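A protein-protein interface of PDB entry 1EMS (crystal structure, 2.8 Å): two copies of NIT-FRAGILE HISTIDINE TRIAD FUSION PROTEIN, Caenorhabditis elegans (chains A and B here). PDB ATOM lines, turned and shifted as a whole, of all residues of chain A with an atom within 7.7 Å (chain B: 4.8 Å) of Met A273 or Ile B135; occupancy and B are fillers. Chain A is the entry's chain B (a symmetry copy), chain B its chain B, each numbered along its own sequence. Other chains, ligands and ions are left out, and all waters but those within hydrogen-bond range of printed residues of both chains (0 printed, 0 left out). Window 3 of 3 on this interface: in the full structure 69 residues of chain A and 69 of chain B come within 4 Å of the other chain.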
ATOM      1  N   GLN A 216      38.053 -14.963  21.293  1.00  0.00           N
ATOM      2  CA  GLN A 216      38.148 -14.433  19.947  1.00  0.00           C
ATOM      3  C   GLN A 216      38.850 -13.083  19.977  1.00  0.00           C
ATOM      4  O   GLN A 216      38.275 -12.065  19.572  1.00  0.00           O
ATOM      5  CB  GLN A 216      36.760 -14.262  19.361  1.00  0.00           C
ATOM      6  CG  GLN A 216      35.903 -15.478  19.523  1.00  0.00           C
ATOM      7  CD  GLN A 216      34.475 -15.211  19.135  1.00  0.00           C
ATOM      8  OE1 GLN A 216      33.824 -14.337  19.709  1.00  0.00           O
ATOM      9  NE2 GLN A 216      33.973 -15.959  18.159  1.00  0.00           N
ATOM     10  N   TRP A 244      41.589 -16.530  15.892  1.00  0.00           N
ATOM     11  CA  TRP A 244      41.182 -17.867  15.463  1.00  0.00           C
ATOM     12  C   TRP A 244      42.097 -18.906  16.083  1.00  0.00           C
ATOM     13  O   TRP A 244      41.871 -20.104  15.925  1.00  0.00           O
ATOM     14  CB  TRP A 244      41.233 -17.979  13.933  1.00  0.00           C
ATOM     15  CG  TRP A 244      40.464 -19.148  13.365  1.00  0.00           C
ATOM     16  CD1 TRP A 244      40.951 -20.137  12.558  1.00  0.00           C
ATOM     17  CD2 TRP A 244      39.070 -19.432  13.550  1.00  0.00           C
ATOM     18  NE1 TRP A 244      39.948 -21.019  12.230  1.00  0.00           N
ATOM     19  CE2 TRP A 244      38.784 -20.611  12.828  1.00  0.00           C
ATOM     20  CE3 TRP A 244      38.034 -18.806  14.256  1.00  0.00           C
ATOM     21  CZ2 TRP A 244      37.503 -21.180  12.793  1.00  0.00           C
ATOM     22  CZ3 TRP A 244      36.754 -19.375  14.220  1.00  0.00           C
ATOM     23  CH2 TRP A 244      36.504 -20.547  13.494  1.00  0.00           C
ATOM     24  N   VAL A 267      38.614  -9.824  13.727  1.00  0.00           N
ATOM     25  CA  VAL A 267      37.972 -10.072  15.016  1.00  0.00           C
ATOM     26  C   VAL A 267      36.455  -9.975  14.822  1.00  0.00           C
ATOM     27  O   VAL A 267      35.717 -10.911  15.170  1.00  0.00           O
ATOM     28  CB  VAL A 267      38.399  -9.045  16.090  1.00  0.00           C
ATOM     29  CG1 VAL A 267      37.605  -9.274  17.374  1.00  0.00           C
ATOM     30  CG2 VAL A 267      39.891  -9.160  16.363  1.00  0.00           C
ATOM     31  N   ASP A 268      35.996  -8.855  14.255  1.00  0.00           N
ATOM     32  CA  ASP A 268      34.570  -8.665  14.006  1.00  0.00           C
ATOM     33  C   ASP A 268      33.974  -9.813  13.194  1.00  0.00           C
ATOM     34  O   ASP A 268      32.929 -10.352  13.554  1.00  0.00           O
ATOM     35  CB  ASP A 268      34.307  -7.351  13.270  1.00  0.00           C
ATOM     36  CG  ASP A 268      34.523  -6.136  14.148  1.00  0.00           C
ATOM     37  OD1 ASP A 268      34.154  -6.197  15.347  1.00  0.00           O
ATOM     38  OD2 ASP A 268      35.046  -5.114  13.635  1.00  0.00           O
ATOM     39  N   THR A 269      34.629 -10.187  12.099  1.00  0.00           N
ATOM     40  CA  THR A 269      34.119 -11.276  11.267  1.00  0.00           C
ATOM     41  C   THR A 269      33.874 -12.544  12.083  1.00  0.00           C
ATOM     42  O   THR A 269      32.793 -13.125  12.024  1.00  0.00           O
ATOM     43  CB  THR A 269      35.093 -11.645  10.125  1.00  0.00           C
ATOM     44  OG1 THR A 269      35.308 -10.508   9.281  1.00  0.00           O
ATOM     45  CG2 THR A 269      34.513 -12.777   9.296  1.00  0.00           C
ATOM     46  N   LEU A 270      34.885 -12.964  12.843  1.00  0.00           N
ATOM     47  CA  LEU A 270      34.790 -14.172  13.656  1.00  0.00           C
ATOM     48  C   LEU A 270      33.676 -14.093  14.687  1.00  0.00           C
ATOM     49  O   LEU A 270      32.882 -15.021  14.818  1.00  0.00           O
ATOM     50  CB  LEU A 270      36.122 -14.448  14.363  1.00  0.00           C
ATOM     51  CG  LEU A 270      37.325 -14.730  13.461  1.00  0.00           C
ATOM     52  CD1 LEU A 270      38.463 -15.270  14.305  1.00  0.00           C
ATOM     53  CD2 LEU A 270      36.950 -15.740  12.387  1.00  0.00           C
ATOM     54  N   ARG A 271      33.617 -12.985  15.416  1.00  0.00           N
ATOM     55  CA  ARG A 271      32.588 -12.823  16.427  1.00  0.00           C
ATOM     56  C   ARG A 271      31.191 -12.843  15.819  1.00  0.00           C
ATOM     57  O   ARG A 271      30.226 -13.250  16.476  1.00  0.00           O
ATOM     58  CB  ARG A 271      32.819 -11.538  17.214  1.00  0.00           C
ATOM     59  CG  ARG A 271      34.058 -11.604  18.065  1.00  0.00           C
ATOM     60  CD  ARG A 271      34.283 -10.346  18.876  1.00  0.00           C
ATOM     61  NE  ARG A 271      35.554 -10.422  19.594  1.00  0.00           N
ATOM     62  CZ  ARG A 271      36.013  -9.481  20.410  1.00  0.00           C
ATOM     63  NH1 ARG A 271      35.304  -8.384  20.616  1.00  0.00           N
ATOM     64  NH2 ARG A 271      37.181  -9.635  21.015  1.00  0.00           N
ATOM     65  N   GLU A 272      31.082 -12.425  14.562  1.00  0.00           N
ATOM     66  CA  GLU A 272      29.796 -12.422  13.879  1.00  0.00           C
ATOM     67  C   GLU A 272      29.396 -13.825  13.402  1.00  0.00           C
ATOM     68  O   GLU A 272      28.257 -14.250  13.592  1.00  0.00           O
ATOM     69  CB  GLU A 272      29.834 -11.479  12.674  1.00  0.00           C
ATOM     70  CG  GLU A 272      28.546 -11.499  11.866  1.00  0.00           C
ATOM     71  CD  GLU A 272      28.633 -10.685  10.593  1.00  0.00           C
ATOM     72  OE1 GLU A 272      29.424 -11.057   9.697  1.00  0.00           O
ATOM     73  OE2 GLU A 272      27.907  -9.674  10.484  1.00  0.00           O
ATOM     74  N   MET A 273      30.339 -14.536  12.787  1.00  0.00           N
ATOM     75  CA  MET A 273      30.088 -15.877  12.260  1.00  0.00           C
ATOM     76  C   MET A 273      30.095 -16.978  13.311  1.00  0.00           C
ATOM     77  O   MET A 273      29.643 -18.096  13.047  1.00  0.00           O
ATOM     78  CB  MET A 273      31.106 -16.212  11.168  1.00  0.00           C
ATOM     79  CG  MET A 273      31.045 -15.281   9.963  1.00  0.00           C
ATOM     80  SD  MET A 273      29.357 -15.137   9.304  1.00  0.00           S
ATOM     81  CE  MET A 273      29.139 -16.787   8.565  1.00  0.00           C
ATOM     82  N   GLN A 274      30.624 -16.668  14.492  1.00  0.00           N
ATOM     83  CA  GLN A 274      30.674 -17.618  15.601  1.00  0.00           C
ATOM     84  C   GLN A 274      30.345 -16.855  16.877  1.00  0.00           C
ATOM     85  O   GLN A 274      31.228 -16.535  17.674  1.00  0.00           O
ATOM     86  CB  GLN A 274      32.064 -18.243  15.727  1.00  0.00           C
ATOM     87  CG  GLN A 274      32.407 -19.279  14.669  1.00  0.00           C
ATOM     88  CD  GLN A 274      32.922 -20.572  15.282  1.00  0.00           C
ATOM     89  OE1 GLN A 274      33.811 -20.563  16.144  1.00  0.00           O
ATOM     90  NE2 GLN A 274      32.364 -21.692  14.841  1.00  0.00           N
ATOM     91  N   PRO A 275      29.057 -16.555  17.088  1.00  0.00           N
ATOM     92  CA  PRO A 275      28.603 -15.818  18.274  1.00  0.00           C
ATOM     93  C   PRO A 275      28.624 -16.636  19.580  1.00  0.00           C
ATOM     94  O   PRO A 275      27.593 -16.778  20.236  1.00  0.00           O
ATOM     95  CB  PRO A 275      27.192 -15.389  17.870  1.00  0.00           C
ATOM     96  CG  PRO A 275      26.721 -16.567  17.083  1.00  0.00           C
ATOM     97  CD  PRO A 275      27.919 -16.900  16.215  1.00  0.00           C
ATOM     98  N   VAL A 276      29.793 -17.156  19.959  1.00  0.00           N
ATOM     99  CA  VAL A 276      29.906 -17.964  21.178  1.00  0.00           C
ATOM    100  C   VAL A 276      29.407 -17.244  22.425  1.00  0.00           C
ATOM    101  O   VAL A 276      28.688 -17.827  23.233  1.00  0.00           O
ATOM    102  CB  VAL A 276      31.367 -18.450  21.443  1.00  0.00           C
ATOM    103  CG1 VAL A 276      31.741 -19.517  20.449  1.00  0.00           C
ATOM    104  CG2 VAL A 276      32.346 -17.292  21.340  1.00  0.00           C
ATOM    105  N   HIS A 279      25.902 -17.637  23.314  1.00  0.00           N
ATOM    106  CA  HIS A 279      25.508 -19.023  23.519  1.00  0.00           C
ATOM    107  C   HIS A 279      25.687 -19.465  24.963  1.00  0.00           C
ATOM    108  O   HIS A 279      25.286 -20.570  25.325  1.00  0.00           O
ATOM    109  CB  HIS A 279      26.346 -19.922  22.613  1.00  0.00           C
ATOM    110  CG  HIS A 279      26.084 -19.722  21.153  1.00  0.00           C
ATOM    111  ND1 HIS A 279      25.414 -18.623  20.660  1.00  0.00           N
ATOM    112  CD2 HIS A 279      26.410 -20.478  20.078  1.00  0.00           C
ATOM    113  CE1 HIS A 279      25.337 -18.713  19.343  1.00  0.00           C
ATOM    114  NE2 HIS A 279      25.934 -19.829  18.966  1.00  0.00           N
ATOM    115  N   PHE B 131      24.794 -24.502  19.004  1.00  0.00           N
ATOM    116  CA  PHE B 131      25.247 -23.477  18.071  1.00  0.00           C
ATOM    117  C   PHE B 131      24.086 -22.893  17.292  1.00  0.00           C
ATOM    118  O   PHE B 131      23.410 -23.608  16.554  1.00  0.00           O
ATOM    119  CB  PHE B 131      26.249 -24.035  17.073  1.00  0.00           C
ATOM    120  CG  PHE B 131      26.880 -22.979  16.225  1.00  0.00           C
ATOM    121  CD1 PHE B 131      27.826 -22.109  16.768  1.00  0.00           C
ATOM    122  CD2 PHE B 131      26.513 -22.826  14.893  1.00  0.00           C
ATOM    123  CE1 PHE B 131      28.398 -21.094  15.998  1.00  0.00           C
ATOM    124  CE2 PHE B 131      27.080 -21.815  14.114  1.00  0.00           C
ATOM    125  CZ  PHE B 131      28.027 -20.947  14.670  1.00  0.00           C
ATOM    126  N   LEU B 133      23.401 -19.710  14.803  1.00  0.00           N
ATOM    127  CA  LEU B 133      23.863 -18.593  13.997  1.00  0.00           C
ATOM    128  C   LEU B 133      22.729 -18.243  13.044  1.00  0.00           C
ATOM    129  O   LEU B 133      22.237 -19.098  12.295  1.00  0.00           O
ATOM    130  CB  LEU B 133      25.093 -19.008  13.188  1.00  0.00           C
ATOM    131  CG  LEU B 133      26.092 -17.963  12.691  1.00  0.00           C
ATOM    132  CD1 LEU B 133      26.960 -18.617  11.638  1.00  0.00           C
ATOM    133  CD2 LEU B 133      25.400 -16.768  12.107  1.00  0.00           C
ATOM    134  N   GLU B 134      22.304 -16.988  13.081  1.00  0.00           N
ATOM    135  CA  GLU B 134      21.244 -16.544  12.194  1.00  0.00           C
ATOM    136  C   GLU B 134      21.513 -15.121  11.733  1.00  0.00           C
ATOM    137  O   GLU B 134      21.098 -14.161  12.379  1.00  0.00           O
ATOM    138  CB  GLU B 134      19.891 -16.616  12.893  1.00  0.00           C
ATOM    139  CG  GLU B 134      18.729 -16.463  11.938  1.00  0.00           C
ATOM    140  CD  GLU B 134      17.393 -16.657  12.613  1.00  0.00           C
ATOM    141  OE1 GLU B 134      17.013 -15.785  13.427  1.00  0.00           O
ATOM    142  OE2 GLU B 134      16.732 -17.685  12.333  1.00  0.00           O
ATOM    143  N   ILE B 135      22.231 -14.997  10.620  1.00  0.00           N
ATOM    144  CA  ILE B 135      22.555 -13.695  10.053  1.00  0.00           C
ATOM    145  C   ILE B 135      21.568 -13.417   8.925  1.00  0.00           C
ATOM    146  O   ILE B 135      21.629 -14.056   7.870  1.00  0.00           O
ATOM    147  CB  ILE B 135      23.974 -13.671   9.481  1.00  0.00           C
ATOM    148  CG1 ILE B 135      24.975 -14.065  10.567  1.00  0.00           C
ATOM    149  CG2 ILE B 135      24.293 -12.280   8.974  1.00  0.00           C
ATOM    150  CD1 ILE B 135      26.395 -14.158  10.079  1.00  0.00           C
ATOM    151  N   PRO B 136      20.669 -12.434   9.128  1.00  0.00           N
ATOM    152  CA  PRO B 136      19.627 -12.009   8.186  1.00  0.00           C
ATOM    153  C   PRO B 136      19.690 -12.624   6.790  1.00  0.00           C
ATOM    154  O   PRO B 136      19.065 -13.658   6.531  1.00  0.00           O
ATOM    155  CB  PRO B 136      19.761 -10.475   8.176  1.00  0.00           C
ATOM    156  CG  PRO B 136      20.960 -10.169   9.111  1.00  0.00           C
ATOM    157  CD  PRO B 136      20.964 -11.330  10.052  1.00  0.00           C
ATOM    158  N   GLY B 137      20.437 -11.993   5.892  1.00  0.00           N
ATOM    159  CA  GLY B 137      20.543 -12.519   4.546  1.00  0.00           C
ATOM    160  C   GLY B 137      21.958 -12.953   4.253  1.00  0.00           C
ATOM    161  O   GLY B 137      22.634 -12.352   3.422  1.00  0.00           O
ATOM    162  N   LYS B 138      22.417 -13.992   4.940  1.00  0.00           N
ATOM    163  CA  LYS B 138      23.770 -14.491   4.739  1.00  0.00           C
ATOM    164  C   LYS B 138      23.833 -15.989   5.007  1.00  0.00           C
ATOM    165  O   LYS B 138      24.164 -16.775   4.116  1.00  0.00           O
ATOM    166  CB  LYS B 138      24.752 -13.747   5.656  1.00  0.00           C
ATOM    167  CG  LYS B 138      24.722 -12.226   5.488  1.00  0.00           C
ATOM    168  CD  LYS B 138      25.785 -11.522   6.324  1.00  0.00           C
ATOM    169  CE  LYS B 138      25.591 -10.009   6.306  1.00  0.00           C
ATOM    170  NZ  LYS B 138      26.504  -9.324   7.268  1.00  0.00           N
ATOM    171  N   VAL B 139      23.514 -16.381   6.238  1.00  0.00           N
ATOM    172  CA  VAL B 139      23.530 -17.788   6.629  1.00  0.00           C
ATOM    173  C   VAL B 139      22.732 -18.011   7.908  1.00  0.00           C
ATOM    174  O   VAL B 139      22.692 -17.146   8.785  1.00  0.00           O
ATOM    175  CB  VAL B 139      24.987 -18.300   6.814  1.00  0.00           C
ATOM    176  CG1 VAL B 139      25.032 -19.422   7.836  1.00  0.00           C
ATOM    177  CG2 VAL B 139      25.525 -18.810   5.477  1.00  0.00           C
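No position is printed for both chains. Of the 6 pairs that touch across the chains among the printed residues, none has its exchanged pair printed and touching as well.
NZ of Lys B138 lies within salt-bridge range of OE2 of Glu A272, at 3.5 Å.
Among the printed residues, pairs that only touch across the chains: Glu A272 with Ile B135, Met A273 with Phe B131, Met A273 with Leu B133, Met A273 with Ile B135 and His A279 with Phe B131.
The backbone carbonyl oxygen (O) of Pro A275 lies within hydrogen-bond range of a ring nitrogen (ND1) of His A279, at 2.9 Å.
Met A273 touches three residues of chain B. Ile B135 touches just these residues of chain A: Glu A272 (3.9 Å) and Met A273 (3.2 Å). Printed residues of chain A within 4 Å of Lys B138: Glu A272 (3.5 Å). Of the printed residues of chain A, Phe B131 touches Met A273 and His A279. Printed residues of chain B within 4 Å of Glu A272: Ile B135 (3.9 Å) and Lys B138 (3.5 Å). Gln A274 touches none of the printed residues of chain B. Val A267 touches none of the printed residues of chain B. The nearest printed residue of chain B that does not touch Met A273 is Val B139 (4.8 Å). The nearest residue of chain A that does not touch Ile B135 is Gln A274 (6.6 Å).
Of the 8 printed residues of chain B, 4 touch a printed residue of chain A. Printed residues of chain B that touch a printed residue of chain A: Phe B131, Leu B133, Ile B135 and Lys B138. Along chain B the printed residues that touch a printed residue of chain A span positions 131 to 138. Among the printed residues, 6 pairs touch across the chains.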
